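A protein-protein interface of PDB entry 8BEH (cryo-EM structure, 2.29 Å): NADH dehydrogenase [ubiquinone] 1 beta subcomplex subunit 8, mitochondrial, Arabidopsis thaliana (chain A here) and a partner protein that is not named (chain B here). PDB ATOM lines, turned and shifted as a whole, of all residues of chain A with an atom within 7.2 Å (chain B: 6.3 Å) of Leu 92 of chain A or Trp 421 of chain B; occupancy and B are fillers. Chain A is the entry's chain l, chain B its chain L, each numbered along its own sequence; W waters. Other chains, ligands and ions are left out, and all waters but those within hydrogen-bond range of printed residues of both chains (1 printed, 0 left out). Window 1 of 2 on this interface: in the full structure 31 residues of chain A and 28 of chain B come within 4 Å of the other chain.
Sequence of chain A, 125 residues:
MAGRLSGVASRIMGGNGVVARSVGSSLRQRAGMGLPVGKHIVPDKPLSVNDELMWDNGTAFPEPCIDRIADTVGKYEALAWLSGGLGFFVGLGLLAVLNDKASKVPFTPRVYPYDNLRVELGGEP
Among the printed residues, merely in contact across the chains: Leu 92 of chain A with Phe 418 of chain B, Lys 101 of chain A with Asn 417 of chain B, Phe 89 of chain A with Phe 418 of chain B, Leu 92 of chain A with Leu 422 of chain B, Gly 93 of chain A with Phe 418 of chain B, Ala 96 of chain A with Trp 421 of chain B, Phe 89 of chain A with Leu 422 of chain B, Leu 92 of chain A with Trp 421 of chain B and Asn 99 of chain A with Trp 421 of chain B.
The side-chain amide oxygen of Asn 417 of chain B lies within hydrogen-bond range of the side-chain amide nitrogen of Asn 99 of chain A.
O of Leu 422 of chain B sits at hydrogen-bond distance from OG of Ser 426 of chain B, at 2.9 Å.
Water W1 lies within hydrogen-bond range of the side-chain amino group (NZ) of Lys 101 of chain A (3.0 Å), the backbone NH (N) of Asn 417 of chain B (3.2 Å) and the backbone carbonyl oxygen (O) of Gly 416 of chain B (3.3 Å).
Hydrophobic or aromatic side chains of chain A that line the printed part of chain B: Phe 89, Leu 92 and Ala 96. Of the 11 printed residues of chain B, 4 touch a printed residue of chain A. Printed residues of chain B that touch a printed residue of chain A: Asn 417, Phe 418, Trp 421 and Leu 422.
Of the printed residues of chain B, Leu 92 of chain A touches Phe 418, Trp 421 and Leu 422. Of chain A, only Leu 92, Ala 96 and Asn 99 come within 4 Å of Trp 421 of chain B. Of the printed residues of chain A, Leu 422 of chain B touches Phe 89 and Leu 92. Of the printed residues of chain A, Asn 417 of chain B touches Asn 99 (2.9 Å) and Lys 101 (3.6 Å). Printed residues of chain B within 4 Å of Lys 101 of chain A: Asn 417. Ala 419 of chain B touches none of the printed residues of chain A. Leu 95 of chain A touches none of the printed residues of chain B. The nearest printed residue of chain B that does not touch Leu 92 of chain A is Asn 417 of chain B (6.4 Å). The nearest printed residue of chain A that does not touch Phe 418 of chain B is Ala 96 of chain A (4.4 Å).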
ATOM      1  N   LEU A  86      23.478  15.129 -20.740  1.00  0.00           N
ATOM      2  CA  LEU A  86      23.405  15.786 -19.436  1.00  0.00           C
ATOM      3  C   LEU A  86      23.244  17.300 -19.577  1.00  0.00           C
ATOM      4  O   LEU A  86      22.629  17.950 -18.717  1.00  0.00           O
ATOM      5  CB  LEU A  86      24.644  15.439 -18.612  1.00  0.00           C
ATOM      6  CG  LEU A  86      24.830  13.946 -18.311  1.00  0.00           C
ATOM      7  CD1 LEU A  86      25.964  13.710 -17.328  1.00  0.00           C
ATOM      8  CD2 LEU A  86      23.546  13.306 -17.806  1.00  0.00           C
ATOM      9  N   GLY A  87      23.775  17.875 -20.656  1.00  0.00           N
ATOM     10  CA  GLY A  87      23.554  19.282 -20.924  1.00  0.00           C
ATOM     11  C   GLY A  87      22.111  19.589 -21.257  1.00  0.00           C
ATOM     12  O   GLY A  87      21.651  20.710 -21.047  1.00  0.00           O
ATOM     13  N   PHE A  88      21.382  18.603 -21.781  1.00  0.00           N
ATOM     14  CA  PHE A  88      19.927  18.733 -21.868  1.00  0.00           C
ATOM     15  C   PHE A  88      19.313  19.003 -20.495  1.00  0.00           C
ATOM     16  O   PHE A  88      18.484  19.907 -20.340  1.00  0.00           O
ATOM     17  CB  PHE A  88      19.314  17.473 -22.474  1.00  0.00           C
ATOM     18  CG  PHE A  88      17.814  17.472 -22.463  1.00  0.00           C
ATOM     19  CD1 PHE A  88      17.099  18.475 -23.092  1.00  0.00           C
ATOM     20  CD2 PHE A  88      17.119  16.498 -21.764  1.00  0.00           C
ATOM     21  CE1 PHE A  88      15.717  18.480 -23.064  1.00  0.00           C
ATOM     22  CE2 PHE A  88      15.739  16.499 -21.731  1.00  0.00           C
ATOM     23  CZ  PHE A  88      15.037  17.492 -22.383  1.00  0.00           C
ATOM     24  N   PHE A  89      19.697  18.213 -19.487  1.00  0.00           N
ATOM     25  CA  PHE A  89      19.165  18.418 -18.143  1.00  0.00           C
ATOM     26  C   PHE A  89      19.583  19.772 -17.588  1.00  0.00           C
ATOM     27  O   PHE A  89      18.791  20.454 -16.926  1.00  0.00           O
ATOM     28  CB  PHE A  89      19.630  17.299 -17.208  1.00  0.00           C
ATOM     29  CG  PHE A  89      18.995  15.972 -17.484  1.00  0.00           C
ATOM     30  CD1 PHE A  89      17.642  15.876 -17.746  1.00  0.00           C
ATOM     31  CD2 PHE A  89      19.753  14.814 -17.468  1.00  0.00           C
ATOM     32  CE1 PHE A  89      17.058  14.658 -17.995  1.00  0.00           C
ATOM     33  CE2 PHE A  89      19.173  13.590 -17.718  1.00  0.00           C
ATOM     34  CZ  PHE A  89      17.821  13.512 -17.983  1.00  0.00           C
ATOM     35  N   VAL A  90      20.830  20.173 -17.842  1.00  0.00           N
ATOM     36  CA  VAL A  90      21.293  21.486 -17.392  1.00  0.00           C
ATOM     37  C   VAL A  90      20.467  22.596 -18.037  1.00  0.00           C
ATOM     38  O   VAL A  90      20.053  23.552 -17.368  1.00  0.00           O
ATOM     39  CB  VAL A  90      22.797  21.655 -17.680  1.00  0.00           C
ATOM     40  CG1 VAL A  90      23.177  23.131 -17.719  1.00  0.00           C
ATOM     41  CG2 VAL A  90      23.622  20.917 -16.646  1.00  0.00           C
ATOM     42  N   GLY A  91      20.214  22.486 -19.342  1.00  0.00           N
ATOM     43  CA  GLY A  91      19.419  23.491 -20.028  1.00  0.00           C
ATOM     44  C   GLY A  91      17.986  23.540 -19.538  1.00  0.00           C
ATOM     45  O   GLY A  91      17.396  24.615 -19.431  1.00  0.00           O
ATOM     46  N   LEU A  92      17.412  22.378 -19.220  1.00  0.00           N
ATOM     47  CA  LEU A  92      16.071  22.349 -18.643  1.00  0.00           C
ATOM     48  C   LEU A  92      16.044  23.009 -17.268  1.00  0.00           C
ATOM     49  O   LEU A  92      15.093  23.723 -16.933  1.00  0.00           O
ATOM     50  CB  LEU A  92      15.569  20.912 -18.557  1.00  0.00           C
ATOM     51  CG  LEU A  92      14.052  20.750 -18.578  1.00  0.00           C
ATOM     52  CD1 LEU A  92      13.523  20.942 -19.987  1.00  0.00           C
ATOM     53  CD2 LEU A  92      13.649  19.397 -18.023  1.00  0.00           C
ATOM     54  N   GLY A  93      17.080  22.780 -16.459  1.00  0.00           N
ATOM     55  CA  GLY A  93      17.160  23.447 -15.169  1.00  0.00           C
ATOM     56  C   GLY A  93      17.272  24.955 -15.293  1.00  0.00           C
ATOM     57  O   GLY A  93      16.619  25.700 -14.557  1.00  0.00           O
ATOM     58  N   LEU A  94      18.100  25.426 -16.229  1.00  0.00           N
ATOM     59  CA  LEU A  94      18.220  26.865 -16.445  1.00  0.00           C
ATOM     60  C   LEU A  94      16.914  27.447 -16.971  1.00  0.00           C
ATOM     61  O   LEU A  94      16.539  28.570 -16.617  1.00  0.00           O
ATOM     62  CB  LEU A  94      19.367  27.173 -17.405  1.00  0.00           C
ATOM     63  CG  LEU A  94      20.751  26.640 -17.025  1.00  0.00           C
ATOM     64  CD1 LEU A  94      21.690  26.696 -18.216  1.00  0.00           C
ATOM     65  CD2 LEU A  94      21.321  27.406 -15.847  1.00  0.00           C
ATOM     66  N   LEU A  95      16.215  26.700 -17.824  1.00  0.00           N
ATOM     67  CA  LEU A  95      14.911  27.139 -18.298  1.00  0.00           C
ATOM     68  C   LEU A  95      13.917  27.246 -17.152  1.00  0.00           C
ATOM     69  O   LEU A  95      13.107  28.174 -17.112  1.00  0.00           O
ATOM     70  CB  LEU A  95      14.401  26.182 -19.370  1.00  0.00           C
ATOM     71  CG  LEU A  95      14.710  26.633 -20.791  1.00  0.00           C
ATOM     72  CD1 LEU A  95      14.627  25.461 -21.752  1.00  0.00           C
ATOM     73  CD2 LEU A  95      13.762  27.741 -21.196  1.00  0.00           C
ATOM     74  N   ALA A  96      13.955  26.297 -16.215  1.00  0.00           N
ATOM     75  CA  ALA A  96      13.076  26.382 -15.053  1.00  0.00           C
ATOM     76  C   ALA A  96      13.437  27.573 -14.173  1.00  0.00           C
ATOM     77  O   ALA A  96      12.556  28.193 -13.572  1.00  0.00           O
ATOM     78  CB  ALA A  96      13.123  25.082 -14.253  1.00  0.00           C
ATOM     79  N   VAL A  97      14.730  27.890 -14.067  1.00  0.00           N
ATOM     80  CA  VAL A  97      15.139  29.105 -13.361  1.00  0.00           C
ATOM     81  C   VAL A  97      14.554  30.333 -14.046  1.00  0.00           C
ATOM     82  O   VAL A  97      13.976  31.216 -13.399  1.00  0.00           O
ATOM     83  CB  VAL A  97      16.674  29.199 -13.280  1.00  0.00           C
ATOM     84  CG1 VAL A  97      17.092  30.620 -12.937  1.00  0.00           C
ATOM     85  CG2 VAL A  97      17.238  28.207 -12.275  1.00  0.00           C
ATOM     86  N   LEU A  98      14.686  30.401 -15.372  1.00  0.00           N
ATOM     87  CA  LEU A  98      14.188  31.553 -16.115  1.00  0.00           C
ATOM     88  C   LEU A  98      12.671  31.654 -16.034  1.00  0.00           C
ATOM     89  O   LEU A  98      12.119  32.756 -16.091  1.00  0.00           O
ATOM     90  CB  LEU A  98      14.638  31.467 -17.572  1.00  0.00           C
ATOM     91  CG  LEU A  98      15.987  32.089 -17.932  1.00  0.00           C
ATOM     92  CD1 LEU A  98      16.011  32.506 -19.396  1.00  0.00           C
ATOM     93  CD2 LEU A  98      16.316  33.267 -17.028  1.00  0.00           C
ATOM     94  N   ASN A  99      11.987  30.518 -15.888  1.00  0.00           N
ATOM     95  CA  ASN A  99      10.532  30.519 -15.813  1.00  0.00           C
ATOM     96  C   ASN A  99      10.043  31.238 -14.562  1.00  0.00           C
ATOM     97  O   ASN A  99       9.016  31.924 -14.598  1.00  0.00           O
ATOM     98  CB  ASN A  99      10.013  29.082 -15.849  1.00  0.00           C
ATOM     99  CG  ASN A  99       8.555  28.998 -16.241  1.00  0.00           C
ATOM    100  OD1 ASN A  99       8.082  29.771 -17.067  1.00  0.00           O
ATOM    101  ND2 ASN A  99       7.837  28.052 -15.654  1.00  0.00           N
ATOM    102  N   LYS A 101       8.626  30.125 -11.805  1.00  0.00           N
ATOM    103  CA  LYS A 101       7.268  29.691 -11.503  1.00  0.00           C
ATOM    104  C   LYS A 101       6.846  30.097 -10.099  1.00  0.00           C
ATOM    105  O   LYS A 101       5.653  30.275  -9.839  1.00  0.00           O
ATOM    106  CB  LYS A 101       7.159  28.176 -11.673  1.00  0.00           C
ATOM    107  CG  LYS A 101       5.739  27.677 -11.861  1.00  0.00           C
ATOM    108  CD  LYS A 101       5.692  26.172 -11.975  1.00  0.00           C
ATOM    109  CE  LYS A 101       4.339  25.632 -11.554  1.00  0.00           C
ATOM    110  NZ  LYS A 101       3.958  24.460 -12.375  1.00  0.00           N
ATOM    111  N   GLY B 416      10.377  21.807  -8.503  1.00  0.00           N
ATOM    112  CA  GLY B 416       9.020  21.359  -8.775  1.00  0.00           C
ATOM    113  C   GLY B 416       8.651  21.492 -10.240  1.00  0.00           C
ATOM    114  O   GLY B 416       8.074  20.580 -10.833  1.00  0.00           O
ATOM    115  N   ASN B 417       8.988  22.633 -10.841  1.00  0.00           N
ATOM    116  CA  ASN B 417       8.759  22.836 -12.268  1.00  0.00           C
ATOM    117  C   ASN B 417       9.539  21.833 -13.108  1.00  0.00           C
ATOM    118  O   ASN B 417       9.005  21.254 -14.068  1.00  0.00           O
ATOM    119  CB  ASN B 417       9.144  24.268 -12.634  1.00  0.00           C
ATOM    120  CG  ASN B 417       8.515  24.732 -13.919  1.00  0.00           C
ATOM    121  OD1 ASN B 417       9.023  25.639 -14.569  1.00  0.00           O
ATOM    122  ND2 ASN B 417       7.421  24.096 -14.310  1.00  0.00           N
ATOM    123  N   PHE B 418      10.805  21.618 -12.754  1.00  0.00           N
ATOM    124  CA  PHE B 418      11.645  20.649 -13.446  1.00  0.00           C
ATOM    125  C   PHE B 418      11.004  19.264 -13.425  1.00  0.00           C
ATOM    126  O   PHE B 418      10.879  18.599 -14.465  1.00  0.00           O
ATOM    127  CB  PHE B 418      13.021  20.646 -12.774  1.00  0.00           C
ATOM    128  CG  PHE B 418      14.056  19.813 -13.463  1.00  0.00           C
ATOM    129  CD1 PHE B 418      14.766  20.321 -14.539  1.00  0.00           C
ATOM    130  CD2 PHE B 418      14.347  18.539 -13.015  1.00  0.00           C
ATOM    131  CE1 PHE B 418      15.739  19.566 -15.162  1.00  0.00           C
ATOM    132  CE2 PHE B 418      15.322  17.780 -13.633  1.00  0.00           C
ATOM    133  CZ  PHE B 418      16.014  18.294 -14.713  1.00  0.00           C
ATOM    134  N   ALA B 419      10.491  18.816 -12.300  1.00  0.00           N
ATOM    135  CA  ALA B 419       9.885  17.505 -12.092  1.00  0.00           C
ATOM    136  C   ALA B 419       8.554  17.394 -12.820  1.00  0.00           C
ATOM    137  O   ALA B 419       8.302  16.379 -13.438  1.00  0.00           O
ATOM    138  CB  ALA B 419       9.761  17.198 -10.640  1.00  0.00           C
ATOM    139  N   PHE B 420       7.824  18.478 -12.822  1.00  0.00           N
ATOM    140  CA  PHE B 420       6.563  18.443 -13.554  1.00  0.00           C
ATOM    141  C   PHE B 420       6.807  18.235 -15.043  1.00  0.00           C
ATOM    142  O   PHE B 420       6.207  17.346 -15.663  1.00  0.00           O
ATOM    143  CB  PHE B 420       5.769  19.724 -13.314  1.00  0.00           C
ATOM    144  CG  PHE B 420       4.519  19.813 -14.133  1.00  0.00           C
ATOM    145  CD1 PHE B 420       3.492  18.911 -13.942  1.00  0.00           C
ATOM    146  CD2 PHE B 420       4.382  20.779 -15.113  1.00  0.00           C
ATOM    147  CE1 PHE B 420       2.341  18.984 -14.696  1.00  0.00           C
ATOM    148  CE2 PHE B 420       3.230  20.855 -15.871  1.00  0.00           C
ATOM    149  CZ  PHE B 420       2.212  19.955 -15.662  1.00  0.00           C
ATOM    150  N   TRP B 421       7.718  19.020 -15.625  1.00  0.00           N
ATOM    151  CA  TRP B 421       8.029  18.864 -17.046  1.00  0.00           C
ATOM    152  C   TRP B 421       8.515  17.450 -17.360  1.00  0.00           C
ATOM    153  O   TRP B 421       8.008  16.790 -18.285  1.00  0.00           O
ATOM    154  CB  TRP B 421       9.086  19.883 -17.470  1.00  0.00           C
ATOM    155  CG  TRP B 421       8.606  21.295 -17.572  1.00  0.00           C
ATOM    156  CD1 TRP B 421       7.319  21.719 -17.726  1.00  0.00           C
ATOM    157  CD2 TRP B 421       9.416  22.473 -17.550  1.00  0.00           C
ATOM    158  NE1 TRP B 421       7.277  23.087 -17.790  1.00  0.00           N
ATOM    159  CE2 TRP B 421       8.552  23.576 -17.687  1.00  0.00           C
ATOM    160  CE3 TRP B 421      10.791  22.703 -17.423  1.00  0.00           C
ATOM    161  CZ2 TRP B 421       9.014  24.888 -17.700  1.00  0.00           C
ATOM    162  CZ3 TRP B 421      11.247  24.006 -17.433  1.00  0.00           C
ATOM    163  CH2 TRP B 421      10.363  25.082 -17.572  1.00  0.00           C
ATOM    164  N   LEU B 422       9.503  16.968 -16.595  1.00  0.00           N
ATOM    165  CA  LEU B 422      10.119  15.688 -16.928  1.00  0.00           C
ATOM    166  C   LEU B 422       9.140  14.529 -16.759  1.00  0.00           C
ATOM    167  O   LEU B 422       9.052  13.661 -17.632  1.00  0.00           O
ATOM    168  CB  LEU B 422      11.378  15.477 -16.092  1.00  0.00           C
ATOM    169  CG  LEU B 422      12.636  16.110 -16.693  1.00  0.00           C
ATOM    170  CD1 LEU B 422      13.890  15.627 -15.984  1.00  0.00           C
ATOM    171  CD2 LEU B 422      12.729  15.838 -18.192  1.00  0.00           C
ATOM    172  N   GLY B 423       8.384  14.504 -15.657  1.00  0.00           N
ATOM    173  CA  GLY B 423       7.386  13.465 -15.480  1.00  0.00           C
ATOM    174  C   GLY B 423       6.304  13.490 -16.539  1.00  0.00           C
ATOM    175  O   GLY B 423       5.873  12.432 -17.021  1.00  0.00           O
ATOM    176  N   SER B 424       5.869  14.689 -16.940  1.00  0.00           N
ATOM    177  CA  SER B 424       4.858  14.793 -17.986  1.00  0.00           C
ATOM    178  C   SER B 424       5.342  14.166 -19.287  1.00  0.00           C
ATOM    179  O   SER B 424       4.641  13.342 -19.883  1.00  0.00           O
ATOM    180  CB  SER B 424       4.472  16.258 -18.194  1.00  0.00           C
ATOM    181  OG  SER B 424       4.152  16.875 -16.961  1.00  0.00           O
ATOM    182  N   VAL B 425       6.549  14.520 -19.737  1.00  0.00           N
ATOM    183  CA  VAL B 425       7.018  13.935 -20.998  1.00  0.00           C
ATOM    184  C   VAL B 425       7.297  12.434 -20.839  1.00  0.00           C
ATOM    185  O   VAL B 425       7.092  11.635 -21.781  1.00  0.00           O
ATOM    186  CB  VAL B 425       8.237  14.716 -21.532  1.00  0.00           C
ATOM    187  CG1 VAL B 425       9.462  14.513 -20.660  1.00  0.00           C
ATOM    188  CG2 VAL B 425       8.524  14.337 -22.977  1.00  0.00           C
ATOM    189  N   SER B 426       7.731  12.015 -19.648  1.00  0.00           N
ATOM    190  CA  SER B 426       7.997  10.604 -19.427  1.00  0.00           C
ATOM    191  C   SER B 426       6.726   9.775 -19.523  1.00  0.00           C
ATOM    192  O   SER B 426       6.789   8.600 -19.884  1.00  0.00           O
ATOM    193  CB  SER B 426       8.672  10.402 -18.072  1.00  0.00           C
ATOM    194  OG  SER B 426       9.976  10.951 -18.082  1.00  0.00           O
HETATM  195  O   HOH W   1       5.862  22.970 -10.605  1.00  0.00           O
